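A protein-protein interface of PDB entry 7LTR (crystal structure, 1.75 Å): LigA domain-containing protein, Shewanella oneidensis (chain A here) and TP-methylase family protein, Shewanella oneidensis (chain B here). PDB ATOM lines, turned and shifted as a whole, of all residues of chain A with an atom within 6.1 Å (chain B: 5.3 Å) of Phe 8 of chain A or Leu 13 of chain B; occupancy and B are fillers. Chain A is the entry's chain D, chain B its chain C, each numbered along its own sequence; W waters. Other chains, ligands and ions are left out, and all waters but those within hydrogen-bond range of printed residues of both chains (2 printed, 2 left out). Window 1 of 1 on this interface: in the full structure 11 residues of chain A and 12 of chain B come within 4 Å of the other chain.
O of Asn 210 of chain B lies within hydrogen-bond range of N of Leu 13 of chain B.
The backbone carbonyl oxygen of Ser 5 of chain A lies within hydrogen-bond range of the side-chain hydroxyl of Thr 9 of chain A, at 3.4 Å.
Among the printed residues, pairs that only touch across the chains: Gly 12 of chain A with Gly 15 of chain B, Gln 13 of chain A with Ala 14 of chain B, Thr 9 of chain A with Ala 14 of chain B, Phe 8 of chain A with Pro 212 of chain B, Phe 8 of chain A with Phe 39 of chain B, Gly 12 of chain A with Leu 13 of chain B, Leu 11 of chain A with Ile 213 of chain B, Phe 8 of chain A with Leu 13 of chain B, Phe 8 of chain A with Ile 213 of chain B, Thr 9 of chain A with Trp 43 of chain B, Leu 11 of chain A with Pro 212 of chain B, Gln 13 of chain A with Trp 43 of chain B, Val 42 of chain A with Ile 213 of chain B and Thr 9 of chain A with Leu 13 of chain B.
Phe 8 of chain A touches just these residues of chain B: Leu 13, Phe 39, Pro 212 and Ile 213.
Printed residues of chain B within 4 Å of Thr 9 of chain A: Leu 13 (3.98 Å), Ala 14 (3.5 Å) and Trp 43 (3.8 Å).
Of the printed residues of chain B, Leu 11 of chain A touches Pro 212 and Ile 213.
Of the printed residues of chain B, Val 42 of chain A touches Ile 213.
Leu 13 of chain B touches just these residues of chain A: Phe 8 (3.7 Å), Thr 9 (3.98 Å) and Gly 12 (3.6 Å).
Printed residues of chain A within 4 Å of Gly 15 of chain B: Gly 12.
Ser 40 of chain B touches none of the printed residues of chain A.
Printed residues of chain A within 4 Å of Trp 43 of chain B: Thr 9 (3.8 Å) and Gln 13 (3.9 Å).
The nearest residue of chain B that does not touch Phe 8 of chain A is Leu 211 of chain B (4.6 Å).
The nearest residue of chain A that does not touch Leu 13 of chain B is Gln 13 of chain A (4.9 Å).
Of the 13 printed residues of chain B, 7 touch a printed residue of chain A.
Hydrophobic or aromatic side chains of chain B within 4 Å of the printed part of chain A: Leu 13, Ala 14, Phe 39, Trp 43, Pro 212 and Ile 213.
Printed residues of chain A that touch a printed residue of chain B: Phe 8, Thr 9, Leu 11, Gly 12, Gln 13 and Val 42.
Among the printed residues, 14 pairs touch across the chains.
Among the printed residues, no Asp or Glu carboxylate lies within 4 Å of a Lys or Arg side-chain nitrogen of the other chain.
Water W2 bridges O of Val 42 of chain A and O of Ile 213 of chain B.
Water W1 lies within hydrogen-bond range of OG1 of Thr 9 of chain A (2.8 Å), OG of Ser 5 of chain A (2.9 Å) and O of Phe 39 of chain B (3.3 Å).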
ATOM      1  N   LEU A   4      25.884 -18.421  -5.691  1.00  0.00           N
ATOM      2  CA  LEU A   4      26.043 -18.840  -7.113  1.00  0.00           C
ATOM      3  C   LEU A   4      25.230 -17.904  -8.012  1.00  0.00           C
ATOM      4  O   LEU A   4      25.793 -17.392  -8.998  1.00  0.00           O
ATOM      5  CB  LEU A   4      25.583 -20.292  -7.269  1.00  0.00           C
ATOM      6  CG  LEU A   4      25.739 -20.882  -8.670  1.00  0.00           C
ATOM      7  CD1 LEU A   4      27.203 -20.932  -9.084  1.00  0.00           C
ATOM      8  CD2 LEU A   4      25.121 -22.269  -8.745  1.00  0.00           C
ATOM      9  N   SER A   5      23.952 -17.687  -7.691  1.00  0.00           N
ATOM     10  CA  SER A   5      23.077 -16.744  -8.429  1.00  0.00           C
ATOM     11  C   SER A   5      23.690 -15.340  -8.367  1.00  0.00           C
ATOM     12  O   SER A   5      23.776 -14.685  -9.426  1.00  0.00           O
ATOM     13  CB  SER A   5      21.663 -16.772  -7.904  1.00  0.00           C
ATOM     14  OG  SER A   5      20.829 -15.914  -8.671  1.00  0.00           O
ATOM     15  N   ASP A   6      24.142 -14.911  -7.184  1.00  0.00           N
ATOM     16  CA  ASP A   6      24.763 -13.575  -6.968  1.00  0.00           C
ATOM     17  C   ASP A   6      26.001 -13.445  -7.862  1.00  0.00           C
ATOM     18  O   ASP A   6      26.196 -12.362  -8.456  1.00  0.00           O
ATOM     19  CB  ASP A   6      25.133 -13.348  -5.499  1.00  0.00           C
ATOM     20  CG  ASP A   6      23.946 -13.042  -4.602  1.00  0.00           C
ATOM     21  OD1 ASP A   6      22.824 -12.921  -5.133  1.00  0.00           O
ATOM     22  OD2 ASP A   6      24.159 -12.924  -3.378  1.00  0.00           O
ATOM     23  N   PHE A   7      26.809 -14.506  -7.952  1.00  0.00           N
ATOM     24  CA  PHE A   7      28.051 -14.525  -8.767  1.00  0.00           C
ATOM     25  C   PHE A   7      27.701 -14.377 -10.252  1.00  0.00           C
ATOM     26  O   PHE A   7      28.309 -13.530 -10.926  1.00  0.00           O
ATOM     27  CB  PHE A   7      28.871 -15.797  -8.544  1.00  0.00           C
ATOM     28  CG  PHE A   7      30.065 -15.875  -9.462  1.00  0.00           C
ATOM     29  CD1 PHE A   7      31.113 -14.978  -9.326  1.00  0.00           C
ATOM     30  CD2 PHE A   7      30.118 -16.803 -10.487  1.00  0.00           C
ATOM     31  CE1 PHE A   7      32.206 -15.031 -10.179  1.00  0.00           C
ATOM     32  CE2 PHE A   7      31.212 -16.859 -11.335  1.00  0.00           C
ATOM     33  CZ  PHE A   7      32.250 -15.969 -11.183  1.00  0.00           C
ATOM     34  N   PHE A   8      26.747 -15.167 -10.752  1.00  0.00           N
ATOM     35  CA  PHE A   8      26.342 -15.156 -12.182  1.00  0.00           C
ATOM     36  C   PHE A   8      25.806 -13.766 -12.553  1.00  0.00           C
ATOM     37  O   PHE A   8      26.133 -13.281 -13.653  1.00  0.00           O
ATOM     38  CB  PHE A   8      25.328 -16.261 -12.484  1.00  0.00           C
ATOM     39  CG  PHE A   8      25.914 -17.647 -12.581  1.00  0.00           C
ATOM     40  CD1 PHE A   8      27.285 -17.845 -12.557  1.00  0.00           C
ATOM     41  CD2 PHE A   8      25.090 -18.750 -12.725  1.00  0.00           C
ATOM     42  CE1 PHE A   8      27.818 -19.122 -12.651  1.00  0.00           C
ATOM     43  CE2 PHE A   8      25.624 -20.025 -12.828  1.00  0.00           C
ATOM     44  CZ  PHE A   8      26.987 -20.208 -12.788  1.00  0.00           C
ATOM     45  N   THR A   9      25.023 -13.136 -11.669  1.00  0.00           N
ATOM     46  CA  THR A   9      24.490 -11.760 -11.869  1.00  0.00           C
ATOM     47  C   THR A   9      25.655 -10.767 -11.987  1.00  0.00           C
ATOM     48  O   THR A   9      25.665  -9.978 -12.956  1.00  0.00           O
ATOM     49  CB  THR A   9      23.538 -11.340 -10.741  1.00  0.00           C
ATOM     50  OG1 THR A   9      22.292 -12.011 -10.927  1.00  0.00           O
ATOM     51  CG2 THR A   9      23.305  -9.845 -10.706  1.00  0.00           C
ATOM     52  N   GLN A  10      26.594 -10.791 -11.038  1.00  0.00           N
ATOM     53  CA  GLN A  10      27.770  -9.879 -11.025  1.00  0.00           C
ATOM     54  C   GLN A  10      28.572 -10.077 -12.315  1.00  0.00           C
ATOM     55  O   GLN A  10      28.932  -9.075 -12.949  1.00  0.00           O
ATOM     56  CB  GLN A  10      28.694 -10.148  -9.837  1.00  0.00           C
ATOM     57  CG  GLN A  10      28.273  -9.479  -8.538  1.00  0.00           C
ATOM     58  CD  GLN A  10      29.368  -9.596  -7.504  1.00  0.00           C
ATOM     59  OE1 GLN A  10      30.531  -9.290  -7.764  1.00  0.00           O
ATOM     60  NE2 GLN A  10      29.004 -10.060  -6.320  1.00  0.00           N
ATOM     61  N   LEU A  11      28.858 -11.333 -12.664  1.00  0.00           N
ATOM     62  CA  LEU A  11      29.680 -11.704 -13.846  1.00  0.00           C
ATOM     63  C   LEU A  11      29.004 -11.178 -15.120  1.00  0.00           C
ATOM     64  O   LEU A  11      29.718 -10.734 -16.045  1.00  0.00           O
ATOM     65  CB  LEU A  11      29.828 -13.228 -13.874  1.00  0.00           C
ATOM     66  CG  LEU A  11      30.694 -13.796 -14.997  1.00  0.00           C
ATOM     67  CD1 LEU A  11      32.083 -13.177 -14.985  1.00  0.00           C
ATOM     68  CD2 LEU A  11      30.784 -15.310 -14.882  1.00  0.00           C
ATOM     69  N   GLY A  12      27.671 -11.207 -15.157  1.00  0.00           N
ATOM     70  CA  GLY A  12      26.878 -10.793 -16.327  1.00  0.00           C
ATOM     71  C   GLY A  12      26.899  -9.285 -16.523  1.00  0.00           C
ATOM     72  O   GLY A  12      26.760  -8.852 -17.676  1.00  0.00           O
ATOM     73  N   GLN A  13      27.075  -8.517 -15.442  1.00  0.00           N
ATOM     74  CA  GLN A  13      26.870  -7.041 -15.415  1.00  0.00           C
ATOM     75  C   GLN A  13      28.195  -6.275 -15.427  1.00  0.00           C
ATOM     76  O   GLN A  13      28.175  -5.093 -15.814  1.00  0.00           O
ATOM     77  CB  GLN A  13      26.175  -6.587 -14.131  1.00  0.00           C
ATOM     78  CG  GLN A  13      24.785  -7.149 -13.918  1.00  0.00           C
ATOM     79  CD  GLN A  13      24.248  -6.697 -12.583  1.00  0.00           C
ATOM     80  OE1 GLN A  13      24.998  -6.502 -11.625  1.00  0.00           O
ATOM     81  NE2 GLN A  13      22.942  -6.517 -12.509  1.00  0.00           N
ATOM     82  N   MET A  29      36.240 -17.866  -9.460  1.00  0.00           N
ATOM     83  CA  MET A  29      35.089 -18.578  -8.840  1.00  0.00           C
ATOM     84  C   MET A  29      35.431 -18.944  -7.388  1.00  0.00           C
ATOM     85  O   MET A  29      34.539 -18.810  -6.526  1.00  0.00           O
ATOM     86  CB  MET A  29      34.702 -19.825  -9.639  1.00  0.00           C
ATOM     87  CG  MET A  29      33.891 -19.488 -10.880  1.00  0.00           C
ATOM     88  SD  MET A  29      33.144 -20.914 -11.700  1.00  0.00           S
ATOM     89  CE  MET A  29      34.533 -21.513 -12.660  1.00  0.00           C
ATOM     90  N   LEU A  34      32.570 -19.876  -4.484  1.00  0.00           N
ATOM     91  CA  LEU A  34      31.822 -21.000  -5.109  1.00  0.00           C
ATOM     92  C   LEU A  34      32.391 -22.324  -4.590  1.00  0.00           C
ATOM     93  O   LEU A  34      33.592 -22.365  -4.251  1.00  0.00           O
ATOM     94  CB  LEU A  34      31.913 -20.919  -6.635  1.00  0.00           C
ATOM     95  CG  LEU A  34      30.785 -20.143  -7.312  1.00  0.00           C
ATOM     96  CD1 LEU A  34      30.827 -18.678  -6.916  1.00  0.00           C
ATOM     97  CD2 LEU A  34      30.851 -20.296  -8.823  1.00  0.00           C
ATOM     98  N   VAL A  42      30.360 -25.719 -13.568  1.00  0.00           N
ATOM     99  CA  VAL A  42      30.580 -24.555 -14.478  1.00  0.00           C
ATOM    100  C   VAL A  42      31.586 -24.959 -15.559  1.00  0.00           C
ATOM    101  O   VAL A  42      31.265 -24.800 -16.752  1.00  0.00           O
ATOM    102  CB  VAL A  42      31.064 -23.309 -13.714  1.00  0.00           C
ATOM    103  CG1 VAL A  42      31.576 -22.236 -14.663  1.00  0.00           C
ATOM    104  CG2 VAL A  42      29.977 -22.754 -12.805  1.00  0.00           C
ATOM    105  N   LEU A  50      23.884 -27.336 -12.360  1.00  0.00           N
ATOM    106  CA  LEU A  50      23.875 -25.937 -11.850  1.00  0.00           C
ATOM    107  C   LEU A  50      22.491 -25.623 -11.268  1.00  0.00           C
ATOM    108  O   LEU A  50      22.421 -24.820 -10.318  1.00  0.00           O
ATOM    109  CB  LEU A  50      24.235 -24.962 -12.977  1.00  0.00           C
ATOM    110  CG  LEU A  50      25.727 -24.810 -13.277  1.00  0.00           C
ATOM    111  CD1 LEU A  50      25.950 -23.834 -14.421  1.00  0.00           C
ATOM    112  CD2 LEU A  50      26.493 -24.362 -12.042  1.00  0.00           C
ATOM    113  N   LEU B  11      19.039 -11.353 -23.900  1.00  0.00           N
ATOM    114  CA  LEU B  11      19.254 -12.827 -23.836  1.00  0.00           C
ATOM    115  C   LEU B  11      20.159 -13.186 -22.651  1.00  0.00           C
ATOM    116  O   LEU B  11      19.853 -14.166 -21.939  1.00  0.00           O
ATOM    117  CB  LEU B  11      19.888 -13.296 -25.149  1.00  0.00           C
ATOM    118  CG  LEU B  11      18.926 -13.556 -26.307  1.00  0.00           C
ATOM    119  CD1 LEU B  11      18.181 -14.866 -26.112  1.00  0.00           C
ATOM    120  CD2 LEU B  11      17.952 -12.403 -26.484  1.00  0.00           C
ATOM    121  N   GLN B  12      21.250 -12.443 -22.465  1.00  0.00           N
ATOM    122  CA  GLN B  12      22.272 -12.717 -21.419  1.00  0.00           C
ATOM    123  C   GLN B  12      21.788 -12.202 -20.059  1.00  0.00           C
ATOM    124  O   GLN B  12      21.278 -11.068 -19.997  1.00  0.00           O
ATOM    125  CB  GLN B  12      23.610 -12.086 -21.798  1.00  0.00           C
ATOM    126  CG  GLN B  12      24.514 -13.017 -22.590  1.00  0.00           C
ATOM    127  CD  GLN B  12      25.071 -14.153 -21.765  1.00  0.00           C
ATOM    128  OE1 GLN B  12      24.749 -14.327 -20.591  1.00  0.00           O
ATOM    129  NE2 GLN B  12      25.930 -14.943 -22.387  1.00  0.00           N
ATOM    130  N   LEU B  13      21.969 -13.016 -19.015  1.00  0.00           N
ATOM    131  CA  LEU B  13      21.594 -12.717 -17.607  1.00  0.00           C
ATOM    132  C   LEU B  13      22.193 -11.377 -17.162  1.00  0.00           C
ATOM    133  O   LEU B  13      23.421 -11.201 -17.298  1.00  0.00           O
ATOM    134  CB  LEU B  13      22.106 -13.853 -16.716  1.00  0.00           C
ATOM    135  CG  LEU B  13      21.866 -13.678 -15.219  1.00  0.00           C
ATOM    136  CD1 LEU B  13      20.381 -13.748 -14.893  1.00  0.00           C
ATOM    137  CD2 LEU B  13      22.639 -14.725 -14.429  1.00  0.00           C
ATOM    138  N   ALA B  14      21.335 -10.485 -16.655  1.00  0.00           N
ATOM    139  CA  ALA B  14      21.675  -9.277 -15.863  1.00  0.00           C
ATOM    140  C   ALA B  14      22.251  -8.156 -16.736  1.00  0.00           C
ATOM    141  O   ALA B  14      21.903  -6.988 -16.483  1.00  0.00           O
ATOM    142  CB  ALA B  14      22.635  -9.645 -14.759  1.00  0.00           C
ATOM    143  N   GLY B  15      23.126  -8.479 -17.694  1.00  0.00           N
ATOM    144  CA  GLY B  15      23.997  -7.484 -18.350  1.00  0.00           C
ATOM    145  C   GLY B  15      23.401  -6.882 -19.609  1.00  0.00           C
ATOM    146  O   GLY B  15      23.866  -5.796 -20.015  1.00  0.00           O
ATOM    147  N   GLN B  16      22.411  -7.538 -20.221  1.00  0.00           N
ATOM    148  CA  GLN B  16      21.958  -7.190 -21.595  1.00  0.00           C
ATOM    149  C   GLN B  16      20.698  -6.317 -21.550  1.00  0.00           C
ATOM    150  O   GLN B  16      20.282  -5.811 -22.614  1.00  0.00           O
ATOM    151  CB  GLN B  16      21.731  -8.456 -22.417  1.00  0.00           C
ATOM    152  CG  GLN B  16      22.163  -8.296 -23.865  1.00  0.00           C
ATOM    153  CD  GLN B  16      22.447  -9.618 -24.532  1.00  0.00           C
ATOM    154  OE1 GLN B  16      21.621 -10.527 -24.526  1.00  0.00           O
ATOM    155  NE2 GLN B  16      23.626  -9.731 -25.121  1.00  0.00           N
ATOM    156  N   PHE B  39      17.806 -18.559 -12.938  1.00  0.00           N
ATOM    157  CA  PHE B  39      18.776 -17.461 -12.688  1.00  0.00           C
ATOM    158  C   PHE B  39      18.145 -16.136 -13.114  1.00  0.00           C
ATOM    159  O   PHE B  39      18.310 -15.139 -12.393  1.00  0.00           O
ATOM    160  CB  PHE B  39      20.093 -17.724 -13.420  1.00  0.00           C
ATOM    161  CG  PHE B  39      20.899 -18.841 -12.809  1.00  0.00           C
ATOM    162  CD1 PHE B  39      21.373 -18.737 -11.512  1.00  0.00           C
ATOM    163  CD2 PHE B  39      21.158 -20.002 -13.517  1.00  0.00           C
ATOM    164  CE1 PHE B  39      22.101 -19.766 -10.941  1.00  0.00           C
ATOM    165  CE2 PHE B  39      21.890 -21.029 -12.945  1.00  0.00           C
ATOM    166  CZ  PHE B  39      22.360 -20.910 -11.659  1.00  0.00           C
ATOM    167  N   SER B  40      17.442 -16.139 -14.251  1.00  0.00           N
ATOM    168  CA  SER B  40      16.716 -14.959 -14.785  1.00  0.00           C
ATOM    169  C   SER B  40      15.640 -14.545 -13.778  1.00  0.00           C
ATOM    170  O   SER B  40      15.569 -13.347 -13.437  1.00  0.00           O
ATOM    171  CB  SER B  40      16.127 -15.242 -16.142  1.00  0.00           C
ATOM    172  OG  SER B  40      15.808 -14.032 -16.810  1.00  0.00           O
ATOM    173  N   TRP B  43      17.243 -13.202 -10.473  1.00  0.00           N
ATOM    174  CA  TRP B  43      17.790 -11.850 -10.756  1.00  0.00           C
ATOM    175  C   TRP B  43      16.650 -10.825 -10.703  1.00  0.00           C
ATOM    176  O   TRP B  43      16.826  -9.775 -10.053  1.00  0.00           O
ATOM    177  CB  TRP B  43      18.519 -11.831 -12.105  1.00  0.00           C
ATOM    178  CG  TRP B  43      18.714 -10.455 -12.661  1.00  0.00           C
ATOM    179  CD1 TRP B  43      19.729  -9.585 -12.388  1.00  0.00           C
ATOM    180  CD2 TRP B  43      17.850  -9.782 -13.593  1.00  0.00           C
ATOM    181  NE1 TRP B  43      19.558  -8.419 -13.086  1.00  0.00           N
ATOM    182  CE2 TRP B  43      18.415  -8.513 -13.837  1.00  0.00           C
ATOM    183  CE3 TRP B  43      16.661 -10.131 -14.242  1.00  0.00           C
ATOM    184  CZ2 TRP B  43      17.824  -7.594 -14.702  1.00  0.00           C
ATOM    185  CZ3 TRP B  43      16.080  -9.223 -15.098  1.00  0.00           C
ATOM    186  CH2 TRP B  43      16.655  -7.972 -15.323  1.00  0.00           C
ATOM    187  N   ASN B 210      22.671 -17.533 -22.686  1.00  0.00           N
ATOM    188  CA  ASN B 210      21.765 -16.909 -21.688  1.00  0.00           C
ATOM    189  C   ASN B 210      22.506 -16.746 -20.350  1.00  0.00           C
ATOM    190  O   ASN B 210      21.983 -16.044 -19.473  1.00  0.00           O
ATOM    191  CB  ASN B 210      20.513 -17.775 -21.524  1.00  0.00           C
ATOM    192  CG  ASN B 210      19.919 -18.194 -22.854  1.00  0.00           C
ATOM    193  OD1 ASN B 210      19.342 -17.373 -23.565  1.00  0.00           O
ATOM    194  ND2 ASN B 210      20.058 -19.463 -23.204  1.00  0.00           N
ATOM    195  N   LEU B 211      23.634 -17.446 -20.190  1.00  0.00           N
ATOM    196  CA  LEU B 211      24.481 -17.338 -18.970  1.00  0.00           C
ATOM    197  C   LEU B 211      25.877 -16.877 -19.375  1.00  0.00           C
ATOM    198  O   LEU B 211      26.368 -17.216 -20.450  1.00  0.00           O
ATOM    199  CB  LEU B 211      24.539 -18.677 -18.227  1.00  0.00           C
ATOM    200  CG  LEU B 211      23.242 -19.127 -17.555  1.00  0.00           C
ATOM    201  CD1 LEU B 211      23.443 -20.461 -16.850  1.00  0.00           C
ATOM    202  CD2 LEU B 211      22.732 -18.081 -16.575  1.00  0.00           C
ATOM    203  N   PRO B 212      26.540 -16.064 -18.526  1.00  0.00           N
ATOM    204  CA  PRO B 212      27.861 -15.524 -18.849  1.00  0.00           C
ATOM    205  C   PRO B 212      28.982 -16.575 -18.826  1.00  0.00           C
ATOM    206  O   PRO B 212      30.075 -16.250 -19.234  1.00  0.00           O
ATOM    207  CB  PRO B 212      28.077 -14.459 -17.763  1.00  0.00           C
ATOM    208  CG  PRO B 212      27.231 -14.934 -16.599  1.00  0.00           C
ATOM    209  CD  PRO B 212      26.023 -15.581 -17.238  1.00  0.00           C
ATOM    210  N   ILE B 213      28.688 -17.791 -18.356  1.00  0.00           N
ATOM    211  CA  ILE B 213      29.676 -18.906 -18.215  1.00  0.00           C
ATOM    212  C   ILE B 213      29.529 -19.852 -19.413  1.00  0.00           C
ATOM    213  O   ILE B 213      30.258 -20.858 -19.473  1.00  0.00           O
ATOM    214  CB  ILE B 213      29.486 -19.638 -16.871  1.00  0.00           C
ATOM    215  CG1 ILE B 213      28.040 -20.100 -16.659  1.00  0.00           C
ATOM    216  CG2 ILE B 213      29.960 -18.765 -15.720  1.00  0.00           C
ATOM    217  CD1 ILE B 213      27.704 -21.406 -17.329  1.00  0.00           C
HETATM  218  O   HOH W   1      21.328 -14.595 -11.204  1.00  0.00           O
HETATM  219  O   HOH W   2      29.622 -23.566 -18.552  1.00  0.00           O
